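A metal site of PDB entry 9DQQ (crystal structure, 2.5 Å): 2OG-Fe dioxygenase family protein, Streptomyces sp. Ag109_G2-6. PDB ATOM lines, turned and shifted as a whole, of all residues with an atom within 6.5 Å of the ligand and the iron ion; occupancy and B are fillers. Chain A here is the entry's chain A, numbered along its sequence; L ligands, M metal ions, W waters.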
ATOM      1  N   ARG A  55     -24.992 -19.202 -19.883  1.00  0.00           N
ATOM      2  CA  ARG A  55     -26.023 -18.962 -18.882  1.00  0.00           C
ATOM      3  C   ARG A  55     -27.363 -19.432 -19.440  1.00  0.00           C
ATOM      4  O   ARG A  55     -27.847 -18.881 -20.425  1.00  0.00           O
ATOM      5  CB  ARG A  55     -26.091 -17.489 -18.482  1.00  0.00           C
ATOM      6  CG  ARG A  55     -27.389 -17.113 -17.776  1.00  0.00           C
ATOM      7  CD  ARG A  55     -27.289 -15.791 -17.016  1.00  0.00           C
ATOM      8  NE  ARG A  55     -26.864 -15.996 -15.632  1.00  0.00           N
ATOM      9  CZ  ARG A  55     -26.975 -15.085 -14.665  1.00  0.00           C
ATOM     10  NH1 ARG A  55     -27.484 -13.878 -14.898  1.00  0.00           N
ATOM     11  NH2 ARG A  55     -26.558 -15.380 -13.433  1.00  0.00           N
ATOM     12  N   PHE A 139     -31.604 -20.240 -12.769  1.00  0.00           N
ATOM     13  CA  PHE A 139     -30.317 -19.905 -13.380  1.00  0.00           C
ATOM     14  C   PHE A 139     -29.421 -21.124 -13.363  1.00  0.00           C
ATOM     15  O   PHE A 139     -29.213 -21.723 -12.299  1.00  0.00           O
ATOM     16  CB  PHE A 139     -29.568 -18.781 -12.649  1.00  0.00           C
ATOM     17  CG  PHE A 139     -30.027 -17.423 -12.987  1.00  0.00           C
ATOM     18  CD1 PHE A 139     -30.109 -17.017 -14.310  1.00  0.00           C
ATOM     19  CD2 PHE A 139     -30.385 -16.529 -11.977  1.00  0.00           C
ATOM     20  CE1 PHE A 139     -30.538 -15.747 -14.626  1.00  0.00           C
ATOM     21  CE2 PHE A 139     -30.833 -15.247 -12.297  1.00  0.00           C
ATOM     22  CZ  PHE A 139     -30.903 -14.858 -13.620  1.00  0.00           C
ATOM     23  N   ILE A 141     -25.473 -21.696 -14.339  1.00  0.00           N
ATOM     24  CA  ILE A 141     -24.207 -21.100 -14.738  1.00  0.00           C
ATOM     25  C   ILE A 141     -23.258 -22.202 -15.184  1.00  0.00           C
ATOM     26  O   ILE A 141     -23.002 -23.142 -14.421  1.00  0.00           O
ATOM     27  CB  ILE A 141     -23.584 -20.282 -13.596  1.00  0.00           C
ATOM     28  CG1 ILE A 141     -24.606 -19.310 -13.027  1.00  0.00           C
ATOM     29  CG2 ILE A 141     -22.376 -19.510 -14.107  1.00  0.00           C
ATOM     30  CD1 ILE A 141     -25.019 -18.259 -14.020  1.00  0.00           C
ATOM     31  N   GLU A 154     -20.427 -10.260 -12.874  1.00  0.00           N
ATOM     32  CA  GLU A 154     -21.167  -9.046 -12.553  1.00  0.00           C
ATOM     33  C   GLU A 154     -20.767  -8.551 -11.172  1.00  0.00           C
ATOM     34  O   GLU A 154     -20.575  -9.341 -10.248  1.00  0.00           O
ATOM     35  CB  GLU A 154     -22.690  -9.263 -12.612  1.00  0.00           C
ATOM     36  CG  GLU A 154     -23.465  -7.988 -12.277  1.00  0.00           C
ATOM     37  CD  GLU A 154     -24.966  -8.119 -12.461  1.00  0.00           C
ATOM     38  OE1 GLU A 154     -25.436  -9.192 -12.895  1.00  0.00           O
ATOM     39  OE2 GLU A 154     -25.676  -7.124 -12.154  1.00  0.00           O
ATOM     40  N   HIS A 157     -24.449  -5.343  -6.752  1.00  0.00           N
ATOM     41  CA  HIS A 157     -25.718  -4.811  -7.243  1.00  0.00           C
ATOM     42  C   HIS A 157     -26.827  -5.171  -6.266  1.00  0.00           C
ATOM     43  O   HIS A 157     -26.637  -5.949  -5.329  1.00  0.00           O
ATOM     44  CB  HIS A 157     -26.035  -5.359  -8.636  1.00  0.00           C
ATOM     45  CG  HIS A 157     -26.333  -6.818  -8.662  1.00  0.00           C
ATOM     46  ND1 HIS A 157     -25.353  -7.791  -8.606  1.00  0.00           N
ATOM     47  CD2 HIS A 157     -27.512  -7.480  -8.741  1.00  0.00           C
ATOM     48  CE1 HIS A 157     -25.920  -8.984  -8.654  1.00  0.00           C
ATOM     49  NE2 HIS A 157     -27.229  -8.823  -8.737  1.00  0.00           N
ATOM     50  N   ARG A 158     -27.996  -4.573  -6.491  1.00  0.00           N
ATOM     51  CA  ARG A 158     -29.238  -5.009  -5.866  1.00  0.00           C
ATOM     52  C   ARG A 158     -30.158  -5.530  -6.954  1.00  0.00           C
ATOM     53  O   ARG A 158     -29.957  -5.250  -8.142  1.00  0.00           O
ATOM     54  CB  ARG A 158     -29.916  -3.859  -5.128  1.00  0.00           C
ATOM     55  CG  ARG A 158     -30.430  -2.779  -6.056  1.00  0.00           C
ATOM     56  CD  ARG A 158     -31.222  -1.775  -5.285  1.00  0.00           C
ATOM     57  NE  ARG A 158     -32.288  -2.430  -4.543  1.00  0.00           N
ATOM     58  CZ  ARG A 158     -33.252  -1.778  -3.904  1.00  0.00           C
ATOM     59  NH1 ARG A 158     -33.323  -0.464  -3.912  1.00  0.00           N
ATOM     60  NH2 ARG A 158     -34.170  -2.468  -3.230  1.00  0.00           N
ATOM     61  N   ASP A 159     -31.159  -6.312  -6.569  1.00  0.00           N
ATOM     62  CA  ASP A 159     -32.051  -6.827  -7.597  1.00  0.00           C
ATOM     63  C   ASP A 159     -33.251  -5.927  -7.851  1.00  0.00           C
ATOM     64  O   ASP A 159     -34.039  -6.230  -8.751  1.00  0.00           O
ATOM     65  CB  ASP A 159     -32.501  -8.264  -7.278  1.00  0.00           C
ATOM     66  CG  ASP A 159     -31.361  -9.253  -7.415  1.00  0.00           C
ATOM     67  OD1 ASP A 159     -30.264  -8.838  -7.850  1.00  0.00           O
ATOM     68  OD2 ASP A 159     -31.527 -10.445  -7.093  1.00  0.00           O
ATOM     69  N   ILE A 166     -32.335 -17.083  -2.363  1.00  0.00           N
ATOM     70  CA  ILE A 166     -31.619 -17.898  -3.317  1.00  0.00           C
ATOM     71  C   ILE A 166     -31.439 -19.257  -2.684  1.00  0.00           C
ATOM     72  O   ILE A 166     -31.017 -19.359  -1.531  1.00  0.00           O
ATOM     73  CB  ILE A 166     -30.263 -17.267  -3.745  1.00  0.00           C
ATOM     74  CG1 ILE A 166     -29.456 -18.261  -4.573  1.00  0.00           C
ATOM     75  CG2 ILE A 166     -29.447 -16.813  -2.553  1.00  0.00           C
ATOM     76  CD1 ILE A 166     -28.266 -17.644  -5.237  1.00  0.00           C
ATOM     77  N   GLY A 177     -17.447 -19.412  -6.827  1.00  0.00           N
ATOM     78  CA  GLY A 177     -18.873 -19.147  -6.661  1.00  0.00           C
ATOM     79  C   GLY A 177     -19.266 -18.704  -5.274  1.00  0.00           C
ATOM     80  O   GLY A 177     -20.344 -19.069  -4.793  1.00  0.00           O
ATOM     81  N   GLU A 178     -18.416 -17.920  -4.629  1.00  0.00           N
ATOM     82  CA  GLU A 178     -18.714 -17.367  -3.315  1.00  0.00           C
ATOM     83  C   GLU A 178     -19.685 -16.198  -3.460  1.00  0.00           C
ATOM     84  O   GLU A 178     -19.519 -15.354  -4.344  1.00  0.00           O
ATOM     85  CB  GLU A 178     -17.432 -16.886  -2.632  1.00  0.00           C
ATOM     86  CG  GLU A 178     -16.444 -17.983  -2.268  1.00  0.00           C
ATOM     87  CD  GLU A 178     -15.548 -18.420  -3.430  1.00  0.00           C
ATOM     88  OE1 GLU A 178     -15.732 -17.961  -4.579  1.00  0.00           O
ATOM     89  OE2 GLU A 178     -14.637 -19.221  -3.163  1.00  0.00           O
ATOM     90  N   SER A 179     -20.699 -16.126  -2.612  1.00  0.00           N
ATOM     91  CA  SER A 179     -21.664 -15.037  -2.663  1.00  0.00           C
ATOM     92  C   SER A 179     -21.131 -13.897  -1.797  1.00  0.00           C
ATOM     93  O   SER A 179     -20.740 -14.126  -0.637  1.00  0.00           O
ATOM     94  CB  SER A 179     -23.049 -15.471  -2.157  1.00  0.00           C
ATOM     95  OG  SER A 179     -23.390 -16.758  -2.595  1.00  0.00           O
ATOM     96  N   LEU A 194     -22.740 -21.171  -0.712  1.00  0.00           N
ATOM     97  CA  LEU A 194     -23.743 -22.195  -0.951  1.00  0.00           C
ATOM     98  C   LEU A 194     -23.048 -23.393  -1.582  1.00  0.00           C
ATOM     99  O   LEU A 194     -22.558 -23.306  -2.707  1.00  0.00           O
ATOM    100  CB  LEU A 194     -24.862 -21.640  -1.833  1.00  0.00           C
ATOM    101  CG  LEU A 194     -25.401 -20.293  -1.305  1.00  0.00           C
ATOM    102  CD1 LEU A 194     -26.502 -19.798  -2.195  1.00  0.00           C
ATOM    103  CD2 LEU A 194     -25.899 -20.420   0.111  1.00  0.00           C
ATOM    104  N   MET A 201     -30.137 -18.580   1.194  1.00  0.00           N
ATOM    105  CA  MET A 201     -29.755 -17.267   1.669  1.00  0.00           C
ATOM    106  C   MET A 201     -30.892 -16.290   1.408  1.00  0.00           C
ATOM    107  O   MET A 201     -31.341 -16.171   0.259  1.00  0.00           O
ATOM    108  CB  MET A 201     -28.486 -16.778   0.970  1.00  0.00           C
ATOM    109  CG  MET A 201     -27.935 -15.544   1.621  1.00  0.00           C
ATOM    110  SD  MET A 201     -28.365 -14.062   0.743  1.00  0.00           S
ATOM    111  CE  MET A 201     -27.533 -14.328  -0.816  1.00  0.00           C
ATOM    112  N   TRP A 203     -32.195 -12.184   1.804  1.00  0.00           N
ATOM    113  CA  TRP A 203     -31.615 -10.862   1.974  1.00  0.00           C
ATOM    114  C   TRP A 203     -32.649  -9.759   1.805  1.00  0.00           C
ATOM    115  O   TRP A 203     -33.642  -9.896   1.077  1.00  0.00           O
ATOM    116  CB  TRP A 203     -30.435 -10.635   1.025  1.00  0.00           C
ATOM    117  CG  TRP A 203     -30.760 -10.245  -0.410  1.00  0.00           C
ATOM    118  CD1 TRP A 203     -30.788  -8.977  -0.933  1.00  0.00           C
ATOM    119  CD2 TRP A 203     -31.021 -11.137  -1.514  1.00  0.00           C
ATOM    120  NE1 TRP A 203     -31.049  -9.023  -2.294  1.00  0.00           N
ATOM    121  CE2 TRP A 203     -31.221 -10.342  -2.666  1.00  0.00           C
ATOM    122  CE3 TRP A 203     -31.100 -12.526  -1.639  1.00  0.00           C
ATOM    123  CZ2 TRP A 203     -31.509 -10.883  -3.920  1.00  0.00           C
ATOM    124  CZ3 TRP A 203     -31.400 -13.074  -2.889  1.00  0.00           C
ATOM    125  CH2 TRP A 203     -31.576 -12.252  -4.022  1.00  0.00           C
ATOM    126  N   ASP A 205     -33.160  -6.424   0.051  1.00  0.00           N
ATOM    127  CA  ASP A 205     -32.516  -5.963  -1.172  1.00  0.00           C
ATOM    128  C   ASP A 205     -32.230  -4.452  -1.180  1.00  0.00           C
ATOM    129  O   ASP A 205     -31.482  -3.993  -2.052  1.00  0.00           O
ATOM    130  CB  ASP A 205     -33.374  -6.361  -2.378  1.00  0.00           C
ATOM    131  CG  ASP A 205     -32.657  -6.116  -3.685  1.00  0.00           C
ATOM    132  OD1 ASP A 205     -31.660  -6.816  -3.961  1.00  0.00           O
ATOM    133  OD2 ASP A 205     -33.087  -5.230  -4.438  1.00  0.00           O
ATOM    134  N   HIS A 210     -25.065  -6.980  -3.387  1.00  0.00           N
ATOM    135  CA  HIS A 210     -24.649  -8.369  -3.439  1.00  0.00           C
ATOM    136  C   HIS A 210     -24.028  -8.663  -4.784  1.00  0.00           C
ATOM    137  O   HIS A 210     -24.117  -7.866  -5.727  1.00  0.00           O
ATOM    138  CB  HIS A 210     -25.824  -9.299  -3.116  1.00  0.00           C
ATOM    139  CG  HIS A 210     -26.864  -9.373  -4.198  1.00  0.00           C
ATOM    140  ND1 HIS A 210     -28.034  -8.644  -4.149  1.00  0.00           N
ATOM    141  CD2 HIS A 210     -26.906 -10.075  -5.354  1.00  0.00           C
ATOM    142  CE1 HIS A 210     -28.752  -8.902  -5.230  1.00  0.00           C
ATOM    143  NE2 HIS A 210     -28.095  -9.767  -5.975  1.00  0.00           N
ATOM    144  N   ALA A 211     -23.392  -9.824  -4.865  1.00  0.00           N
ATOM    145  CA  ALA A 211     -22.673 -10.292  -6.035  1.00  0.00           C
ATOM    146  C   ALA A 211     -22.292 -11.738  -5.780  1.00  0.00           C
ATOM    147  O   ALA A 211     -22.314 -12.200  -4.644  1.00  0.00           O
ATOM    148  CB  ALA A 211     -21.433  -9.439  -6.317  1.00  0.00           C
ATOM    149  N   VAL A 212     -21.935 -12.442  -6.839  1.00  0.00           N
ATOM    150  CA  VAL A 212     -21.399 -13.786  -6.700  1.00  0.00           C
ATOM    151  C   VAL A 212     -20.117 -13.886  -7.516  1.00  0.00           C
ATOM    152  O   VAL A 212     -20.022 -13.341  -8.619  1.00  0.00           O
ATOM    153  CB  VAL A 212     -22.421 -14.872  -7.123  1.00  0.00           C
ATOM    154  CG1 VAL A 212     -22.721 -14.813  -8.618  1.00  0.00           C
ATOM    155  CG2 VAL A 212     -21.884 -16.251  -6.757  1.00  0.00           C
ATOM    156  N   ARG A 226     -23.295 -24.620 -11.840  1.00  0.00           N
ATOM    157  CA  ARG A 226     -23.915 -24.159 -10.606  1.00  0.00           C
ATOM    158  C   ARG A 226     -25.378 -23.788 -10.856  1.00  0.00           C
ATOM    159  O   ARG A 226     -25.647 -22.870 -11.641  1.00  0.00           O
ATOM    160  CB  ARG A 226     -23.138 -22.957 -10.043  1.00  0.00           C
ATOM    161  CG  ARG A 226     -23.692 -22.321  -8.775  1.00  0.00           C
ATOM    162  CD  ARG A 226     -22.746 -21.237  -8.228  1.00  0.00           C
ATOM    163  NE  ARG A 226     -23.129 -20.775  -6.899  1.00  0.00           N
ATOM    164  CZ  ARG A 226     -23.871 -19.694  -6.673  1.00  0.00           C
ATOM    165  NH1 ARG A 226     -24.320 -18.941  -7.664  1.00  0.00           N
ATOM    166  NH2 ARG A 226     -24.159 -19.350  -5.414  1.00  0.00           N
ATOM    167  N   VAL A 228     -28.994 -22.460  -9.371  1.00  0.00           N
ATOM    168  CA  VAL A 228     -29.600 -21.704  -8.272  1.00  0.00           C
ATOM    169  C   VAL A 228     -31.025 -21.297  -8.642  1.00  0.00           C
ATOM    170  O   VAL A 228     -31.315 -20.979  -9.799  1.00  0.00           O
ATOM    171  CB  VAL A 228     -28.757 -20.473  -7.887  1.00  0.00           C
ATOM    172  CG1 VAL A 228     -27.330 -20.901  -7.499  1.00  0.00           C
ATOM    173  CG2 VAL A 228     -28.749 -19.434  -9.001  1.00  0.00           C
ATOM    174  N   ILE A 230     -33.692 -18.399  -7.657  1.00  0.00           N
ATOM    175  CA  ILE A 230     -33.707 -17.081  -7.052  1.00  0.00           C
ATOM    176  C   ILE A 230     -35.127 -16.538  -7.098  1.00  0.00           C
ATOM    177  O   ILE A 230     -35.767 -16.579  -8.163  1.00  0.00           O
ATOM    178  CB  ILE A 230     -32.749 -16.090  -7.735  1.00  0.00           C
ATOM    179  CG1 ILE A 230     -31.322 -16.617  -7.715  1.00  0.00           C
ATOM    180  CG2 ILE A 230     -32.807 -14.693  -7.036  1.00  0.00           C
ATOM    181  CD1 ILE A 230     -30.273 -15.541  -8.097  1.00  0.00           C
HETATM  182  C1  LIG L   1     -28.109 -12.817 -10.183  1.00  0.00           C
HETATM  183  O1  LIG L   1     -28.043 -13.745 -11.016  1.00  0.00           O
HETATM  184  O2  LIG L   1     -28.799 -11.775 -10.170  1.00  0.00           O
HETATM  185  C2  LIG L   1     -27.187 -12.986  -8.940  1.00  0.00           C
HETATM  186  O3  LIG L   1     -27.053 -12.059  -8.142  1.00  0.00           O
HETATM  187  C3  LIG L   1     -26.504 -14.318  -8.789  1.00  0.00           C
HETATM  188  C4  LIG L   1     -26.466 -14.800  -7.361  1.00  0.00           C
HETATM  189  C5  LIG L   1     -25.864 -16.197  -7.208  1.00  0.00           C
HETATM  190  O4  LIG L   1     -25.303 -16.494  -6.139  1.00  0.00           O
HETATM  191  O5  LIG L   1     -26.009 -16.918  -8.223  1.00  0.00           O
HETATM  192 FE    FE M   1     -28.655 -10.273  -7.928  1.00  0.00          FE
HETATM  193  O   HOH W   1     -29.317 -12.061  -7.012  1.00  0.00           O
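The backbone NH of Val 228 sits at hydrogen-bond distance from the backbone carbonyl oxygen of Phe 139 (3.0 Å).
O of Met 201 sits at hydrogen-bond distance from N of Ile 166 (2.9 Å).
N of Asp 159 sits at hydrogen-bond distance from OD1 of Asp 205.
The backbone carbonyl oxygen (O) of Arg 226 is in hydrogen-bond range of the backbone NH (N) of Ile 141, at 2.9 Å.
Water W1 lies within hydrogen-bond range of OD2 of Asp 159 and O2 of the ligand.
NH2 of Arg 55 is in salt-bridge range of O1 of the ligand.
An oxygen (O5) of the ligand lies within salt-bridge range of the guanidinium group (NH1) of Arg 226.
Residues that only touch the ligand: Ile 166 (3.3 Å), Phe 139 (3.4 Å), Val 212 (3.5 Å), Val 228 (3.8 Å) and Ile 230 (3.9 Å).
Hydrophobic or aromatic side chains that line the ligand: Phe 139, His 157, Ile 166, His 210, Val 212, Val 228 and Ile 230.
Of the 21 residues printed, 9 come within 4 Å of the ligand.
The iron ion is bound by a ring nitrogen (NE2) of His 210 (2.1 Å), water W1 (2.1 Å), the side-chain carboxylate (OD1) of Asp 159 (2.2 Å), a ring nitrogen (NE2) of His 157 (2.2 Å) and an oxygen (O3) of the ligand (2.4 Å).
Slightly farther from the iron ion lies O2 of the ligand (2.7 Å).
Within 4 Å of the iron ion: His 157, Asp 159 and His 210.
The nearest printed residue that does not touch the iron ion is Trp 203 (5.0 Å).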
